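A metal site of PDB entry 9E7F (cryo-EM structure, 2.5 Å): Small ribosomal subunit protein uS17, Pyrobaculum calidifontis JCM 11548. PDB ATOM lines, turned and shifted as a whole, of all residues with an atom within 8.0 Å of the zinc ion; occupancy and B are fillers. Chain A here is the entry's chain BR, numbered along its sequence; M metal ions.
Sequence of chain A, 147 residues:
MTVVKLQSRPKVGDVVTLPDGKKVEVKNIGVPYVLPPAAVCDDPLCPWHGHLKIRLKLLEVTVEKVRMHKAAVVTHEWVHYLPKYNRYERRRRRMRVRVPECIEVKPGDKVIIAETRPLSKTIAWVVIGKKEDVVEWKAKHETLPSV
Four residues have an atom within 4 Å of the zinc ion: Cys 41, Cys 46, His 49 and Cys 102. The nearest printed residue that does not touch the zinc ion is Pro 100 (4.5 Å).
The zinc ion is bound by a ring nitrogen (ND1) of His 49 (2.0 Å), the side-chain sulfur (SG) of Cys 46 (2.3 Å), the side-chain sulfur (SG) of Cys 41 (2.3 Å) and the side-chain sulfur (SG) of Cys 102 (2.3 Å).
The backbone NH (N) of Trp 48 lies close to the side-chain sulfur (SG) of Cys 46, at 3.3 Å. The backbone NH (N) of Asp 43 lies close to the side-chain sulfur (SG) of Cys 41 (3.3 Å). The side-chain carboxylate (OE1) of Glu 101 sits close to the side-chain sulfur (SG) of Cys 41.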
ATOM      1  N   THR A   2      14.162  26.482  32.163  1.00  0.00           N
ATOM      2  CA  THR A   2      15.335  26.367  31.302  1.00  0.00           C
ATOM      3  C   THR A   2      15.957  24.979  31.411  1.00  0.00           C
ATOM      4  O   THR A   2      16.400  24.399  30.424  1.00  0.00           O
ATOM      5  CB  THR A   2      16.390  27.430  31.638  1.00  0.00           C
ATOM      6  OG1 THR A   2      15.908  28.715  31.240  1.00  0.00           O
ATOM      7  CG2 THR A   2      17.693  27.130  30.911  1.00  0.00           C
ATOM      8  N   VAL A   3      15.988  24.450  32.634  1.00  0.00           N
ATOM      9  CA  VAL A   3      16.362  23.068  32.876  1.00  0.00           C
ATOM     10  C   VAL A   3      15.189  22.387  33.565  1.00  0.00           C
ATOM     11  O   VAL A   3      14.711  22.856  34.603  1.00  0.00           O
ATOM     12  CB  VAL A   3      17.633  22.947  33.720  1.00  0.00           C
ATOM     13  CG1 VAL A   3      17.532  23.794  34.979  1.00  0.00           C
ATOM     14  CG2 VAL A   3      17.881  21.503  34.087  1.00  0.00           C
ATOM     15  N   VAL A  24      11.971  20.004  23.032  1.00  0.00           N
ATOM     16  CA  VAL A  24      13.412  19.830  22.925  1.00  0.00           C
ATOM     17  C   VAL A  24      13.678  18.369  22.602  1.00  0.00           C
ATOM     18  O   VAL A  24      13.196  17.484  23.313  1.00  0.00           O
ATOM     19  CB  VAL A  24      14.144  20.246  24.208  1.00  0.00           C
ATOM     20  CG1 VAL A  24      15.644  20.155  24.009  1.00  0.00           C
ATOM     21  CG2 VAL A  24      13.731  21.642  24.620  1.00  0.00           C
ATOM     22  N   PRO A  37      21.918  13.179  29.135  1.00  0.00           N
ATOM     23  CA  PRO A  37      21.687  13.565  30.533  1.00  0.00           C
ATOM     24  C   PRO A  37      20.271  13.235  30.981  1.00  0.00           C
ATOM     25  O   PRO A  37      19.357  13.063  30.173  1.00  0.00           O
ATOM     26  CB  PRO A  37      21.923  15.081  30.524  1.00  0.00           C
ATOM     27  CG  PRO A  37      21.746  15.501  29.116  1.00  0.00           C
ATOM     28  CD  PRO A  37      22.126  14.337  28.256  1.00  0.00           C
ATOM     29  N   ALA A  39      18.302  15.142  32.544  1.00  0.00           N
ATOM     30  CA  ALA A  39      17.457  16.320  32.473  1.00  0.00           C
ATOM     31  C   ALA A  39      17.684  17.000  31.127  1.00  0.00           C
ATOM     32  O   ALA A  39      18.616  16.653  30.394  1.00  0.00           O
ATOM     33  CB  ALA A  39      17.734  17.290  33.620  1.00  0.00           C
ATOM     34  N   VAL A  40      16.825  17.947  30.814  1.00  0.00           N
ATOM     35  CA  VAL A  40      16.853  18.621  29.522  1.00  0.00           C
ATOM     36  C   VAL A  40      17.007  20.122  29.740  1.00  0.00           C
ATOM     37  O   VAL A  40      16.361  20.698  30.625  1.00  0.00           O
ATOM     38  CB  VAL A  40      15.578  18.330  28.704  1.00  0.00           C
ATOM     39  CG1 VAL A  40      15.452  19.301  27.552  1.00  0.00           C
ATOM     40  CG2 VAL A  40      15.609  16.898  28.195  1.00  0.00           C
ATOM     41  N   CYS A  41      17.876  20.745  28.950  1.00  0.00           N
ATOM     42  CA  CYS A  41      18.018  22.189  28.939  1.00  0.00           C
ATOM     43  C   CYS A  41      17.672  22.710  27.546  1.00  0.00           C
ATOM     44  O   CYS A  41      17.482  21.943  26.606  1.00  0.00           O
ATOM     45  CB  CYS A  41      19.439  22.610  29.323  1.00  0.00           C
ATOM     46  SG  CYS A  41      20.590  22.762  27.959  1.00  0.00           S
ATOM     47  N   ASP A  42      17.577  24.026  27.432  1.00  0.00           N
ATOM     48  CA  ASP A  42      17.247  24.676  26.173  1.00  0.00           C
ATOM     49  C   ASP A  42      18.383  25.546  25.647  1.00  0.00           C
ATOM     50  O   ASP A  42      18.160  26.351  24.734  1.00  0.00           O
ATOM     51  CB  ASP A  42      15.962  25.492  26.313  1.00  0.00           C
ATOM     52  CG  ASP A  42      16.034  26.546  27.414  1.00  0.00           C
ATOM     53  OD1 ASP A  42      15.142  26.537  28.285  1.00  0.00           O
ATOM     54  OD2 ASP A  42      16.938  27.411  27.416  1.00  0.00           O
ATOM     55  N   ASP A  43      19.577  25.416  26.200  1.00  0.00           N
ATOM     56  CA  ASP A  43      20.691  26.247  25.797  1.00  0.00           C
ATOM     57  C   ASP A  43      21.076  25.921  24.360  1.00  0.00           C
ATOM     58  O   ASP A  43      21.333  24.752  24.045  1.00  0.00           O
ATOM     59  CB  ASP A  43      21.878  26.022  26.730  1.00  0.00           C
ATOM     60  CG  ASP A  43      22.821  27.203  26.779  1.00  0.00           C
ATOM     61  OD1 ASP A  43      22.544  28.211  26.108  1.00  0.00           O
ATOM     62  OD2 ASP A  43      23.835  27.126  27.497  1.00  0.00           O
ATOM     63  N   PRO A  44      21.139  26.911  23.462  1.00  0.00           N
ATOM     64  CA  PRO A  44      21.581  26.632  22.091  1.00  0.00           C
ATOM     65  C   PRO A  44      23.028  26.198  21.978  1.00  0.00           C
ATOM     66  O   PRO A  44      23.399  25.639  20.941  1.00  0.00           O
ATOM     67  CB  PRO A  44      21.346  27.974  21.360  1.00  0.00           C
ATOM     68  CG  PRO A  44      21.161  28.981  22.417  1.00  0.00           C
ATOM     69  CD  PRO A  44      20.775  28.313  23.680  1.00  0.00           C
ATOM     70  N   LEU A  45      23.862  26.436  22.993  1.00  0.00           N
ATOM     71  CA  LEU A  45      25.244  25.991  22.984  1.00  0.00           C
ATOM     72  C   LEU A  45      25.419  24.643  23.661  1.00  0.00           C
ATOM     73  O   LEU A  45      26.551  24.208  23.893  1.00  0.00           O
ATOM     74  CB  LEU A  45      26.135  27.029  23.668  1.00  0.00           C
ATOM     75  CG  LEU A  45      26.218  28.407  23.012  1.00  0.00           C
ATOM     76  CD1 LEU A  45      27.042  29.357  23.864  1.00  0.00           C
ATOM     77  CD2 LEU A  45      26.791  28.319  21.613  1.00  0.00           C
ATOM     78  N   CYS A  46      24.326  23.982  24.019  1.00  0.00           N
ATOM     79  CA  CYS A  46      24.388  22.630  24.554  1.00  0.00           C
ATOM     80  C   CYS A  46      24.594  21.622  23.416  1.00  0.00           C
ATOM     81  O   CYS A  46      24.066  21.801  22.319  1.00  0.00           O
ATOM     82  CB  CYS A  46      23.097  22.308  25.297  1.00  0.00           C
ATOM     83  SG  CYS A  46      23.003  20.622  25.930  1.00  0.00           S
ATOM     84  N   PRO A  47      25.365  20.572  23.661  1.00  0.00           N
ATOM     85  CA  PRO A  47      25.553  19.564  22.613  1.00  0.00           C
ATOM     86  C   PRO A  47      24.436  18.539  22.572  1.00  0.00           C
ATOM     87  O   PRO A  47      24.200  17.921  21.533  1.00  0.00           O
ATOM     88  CB  PRO A  47      26.891  18.910  22.984  1.00  0.00           C
ATOM     89  CG  PRO A  47      27.123  19.236  24.408  1.00  0.00           C
ATOM     90  CD  PRO A  47      26.196  20.322  24.847  1.00  0.00           C
ATOM     91  N   TRP A  48      23.725  18.360  23.686  1.00  0.00           N
ATOM     92  CA  TRP A  48      22.595  17.442  23.693  1.00  0.00           C
ATOM     93  C   TRP A  48      21.314  18.094  23.209  1.00  0.00           C
ATOM     94  O   TRP A  48      20.551  17.472  22.459  1.00  0.00           O
ATOM     95  CB  TRP A  48      22.363  16.892  25.107  1.00  0.00           C
ATOM     96  CG  TRP A  48      23.446  16.025  25.589  1.00  0.00           C
ATOM     97  CD1 TRP A  48      24.392  16.348  26.506  1.00  0.00           C
ATOM     98  CD2 TRP A  48      23.703  14.681  25.197  1.00  0.00           C
ATOM     99  NE1 TRP A  48      25.233  15.290  26.706  1.00  0.00           N
ATOM    100  CE2 TRP A  48      24.827  14.245  25.906  1.00  0.00           C
ATOM    101  CE3 TRP A  48      23.097  13.797  24.297  1.00  0.00           C
ATOM    102  CZ2 TRP A  48      25.361  12.969  25.761  1.00  0.00           C
ATOM    103  CZ3 TRP A  48      23.623  12.539  24.155  1.00  0.00           C
ATOM    104  CH2 TRP A  48      24.747  12.135  24.874  1.00  0.00           C
ATOM    105  N   HIS A  49      21.049  19.331  23.633  1.00  0.00           N
ATOM    106  CA  HIS A  49      19.787  19.991  23.364  1.00  0.00           C
ATOM    107  C   HIS A  49      20.003  21.340  22.685  1.00  0.00           C
ATOM    108  O   HIS A  49      19.225  22.264  22.882  1.00  0.00           O
ATOM    109  CB  HIS A  49      18.987  20.165  24.650  1.00  0.00           C
ATOM    110  CG  HIS A  49      19.271  19.115  25.675  1.00  0.00           C
ATOM    111  ND1 HIS A  49      19.998  19.366  26.810  1.00  0.00           N
ATOM    112  CD2 HIS A  49      18.938  17.804  25.720  1.00  0.00           C
ATOM    113  CE1 HIS A  49      20.093  18.263  27.528  1.00  0.00           C
ATOM    114  NE2 HIS A  49      19.468  17.299  26.884  1.00  0.00           N
ATOM    115  N   GLY A  50      21.055  21.449  21.889  1.00  0.00           N
ATOM    116  CA  GLY A  50      21.357  22.692  21.212  1.00  0.00           C
ATOM    117  C   GLY A  50      22.033  22.438  19.891  1.00  0.00           C
ATOM    118  O   GLY A  50      22.050  21.302  19.414  1.00  0.00           O
ATOM    119  N   VAL A  99      30.039  23.572  31.379  1.00  0.00           N
ATOM    120  CA  VAL A  99      29.159  22.641  32.073  1.00  0.00           C
ATOM    121  C   VAL A  99      27.713  22.991  31.743  1.00  0.00           C
ATOM    122  O   VAL A  99      27.201  24.015  32.233  1.00  0.00           O
ATOM    123  CB  VAL A  99      29.401  22.662  33.583  1.00  0.00           C
ATOM    124  CG1 VAL A  99      28.538  21.640  34.269  1.00  0.00           C
ATOM    125  CG2 VAL A  99      30.863  22.400  33.878  1.00  0.00           C
ATOM    126  N   PRO A 100      27.028  22.204  30.922  1.00  0.00           N
ATOM    127  CA  PRO A 100      25.647  22.543  30.560  1.00  0.00           C
ATOM    128  C   PRO A 100      24.709  22.401  31.738  1.00  0.00           C
ATOM    129  O   PRO A 100      24.991  21.727  32.739  1.00  0.00           O
ATOM    130  CB  PRO A 100      25.311  21.532  29.452  1.00  0.00           C
ATOM    131  CG  PRO A 100      26.594  20.882  29.083  1.00  0.00           C
ATOM    132  CD  PRO A 100      27.526  21.021  30.222  1.00  0.00           C
ATOM    133  N   GLU A 101      23.559  23.073  31.622  1.00  0.00           N
ATOM    134  CA  GLU A 101      22.608  23.102  32.724  1.00  0.00           C
ATOM    135  C   GLU A 101      21.988  21.736  32.977  1.00  0.00           C
ATOM    136  O   GLU A 101      21.661  21.397  34.120  1.00  0.00           O
ATOM    137  CB  GLU A 101      21.520  24.135  32.435  1.00  0.00           C
ATOM    138  CG  GLU A 101      22.037  25.536  32.237  1.00  0.00           C
ATOM    139  CD  GLU A 101      21.698  26.079  30.863  1.00  0.00           C
ATOM    140  OE1 GLU A 101      21.459  25.278  29.938  1.00  0.00           O
ATOM    141  OE2 GLU A 101      21.649  27.322  30.712  1.00  0.00           O
ATOM    142  N   CYS A 102      21.827  20.931  31.931  1.00  0.00           N
ATOM    143  CA  CYS A 102      21.251  19.608  32.097  1.00  0.00           C
ATOM    144  C   CYS A 102      22.182  18.630  32.806  1.00  0.00           C
ATOM    145  O   CYS A 102      21.717  17.566  33.235  1.00  0.00           O
ATOM    146  CB  CYS A 102      20.841  19.044  30.738  1.00  0.00           C
ATOM    147  SG  CYS A 102      22.005  19.414  29.415  1.00  0.00           S
ATOM    148  N   ILE A 103      23.468  18.946  32.937  1.00  0.00           N
ATOM    149  CA  ILE A 103      24.434  18.087  33.606  1.00  0.00           C
ATOM    150  C   ILE A 103      24.888  18.784  34.869  1.00  0.00           C
ATOM    151  O   ILE A 103      25.354  19.932  34.820  1.00  0.00           O
ATOM    152  CB  ILE A 103      25.631  17.769  32.703  1.00  0.00           C
ATOM    153  CG1 ILE A 103      25.154  17.253  31.345  1.00  0.00           C
ATOM    154  CG2 ILE A 103      26.524  16.739  33.360  1.00  0.00           C
ATOM    155  CD1 ILE A 103      26.265  16.845  30.437  1.00  0.00           C
HETATM  156 ZN    ZN M   1      21.376  20.634  27.559  1.00  0.00          ZN
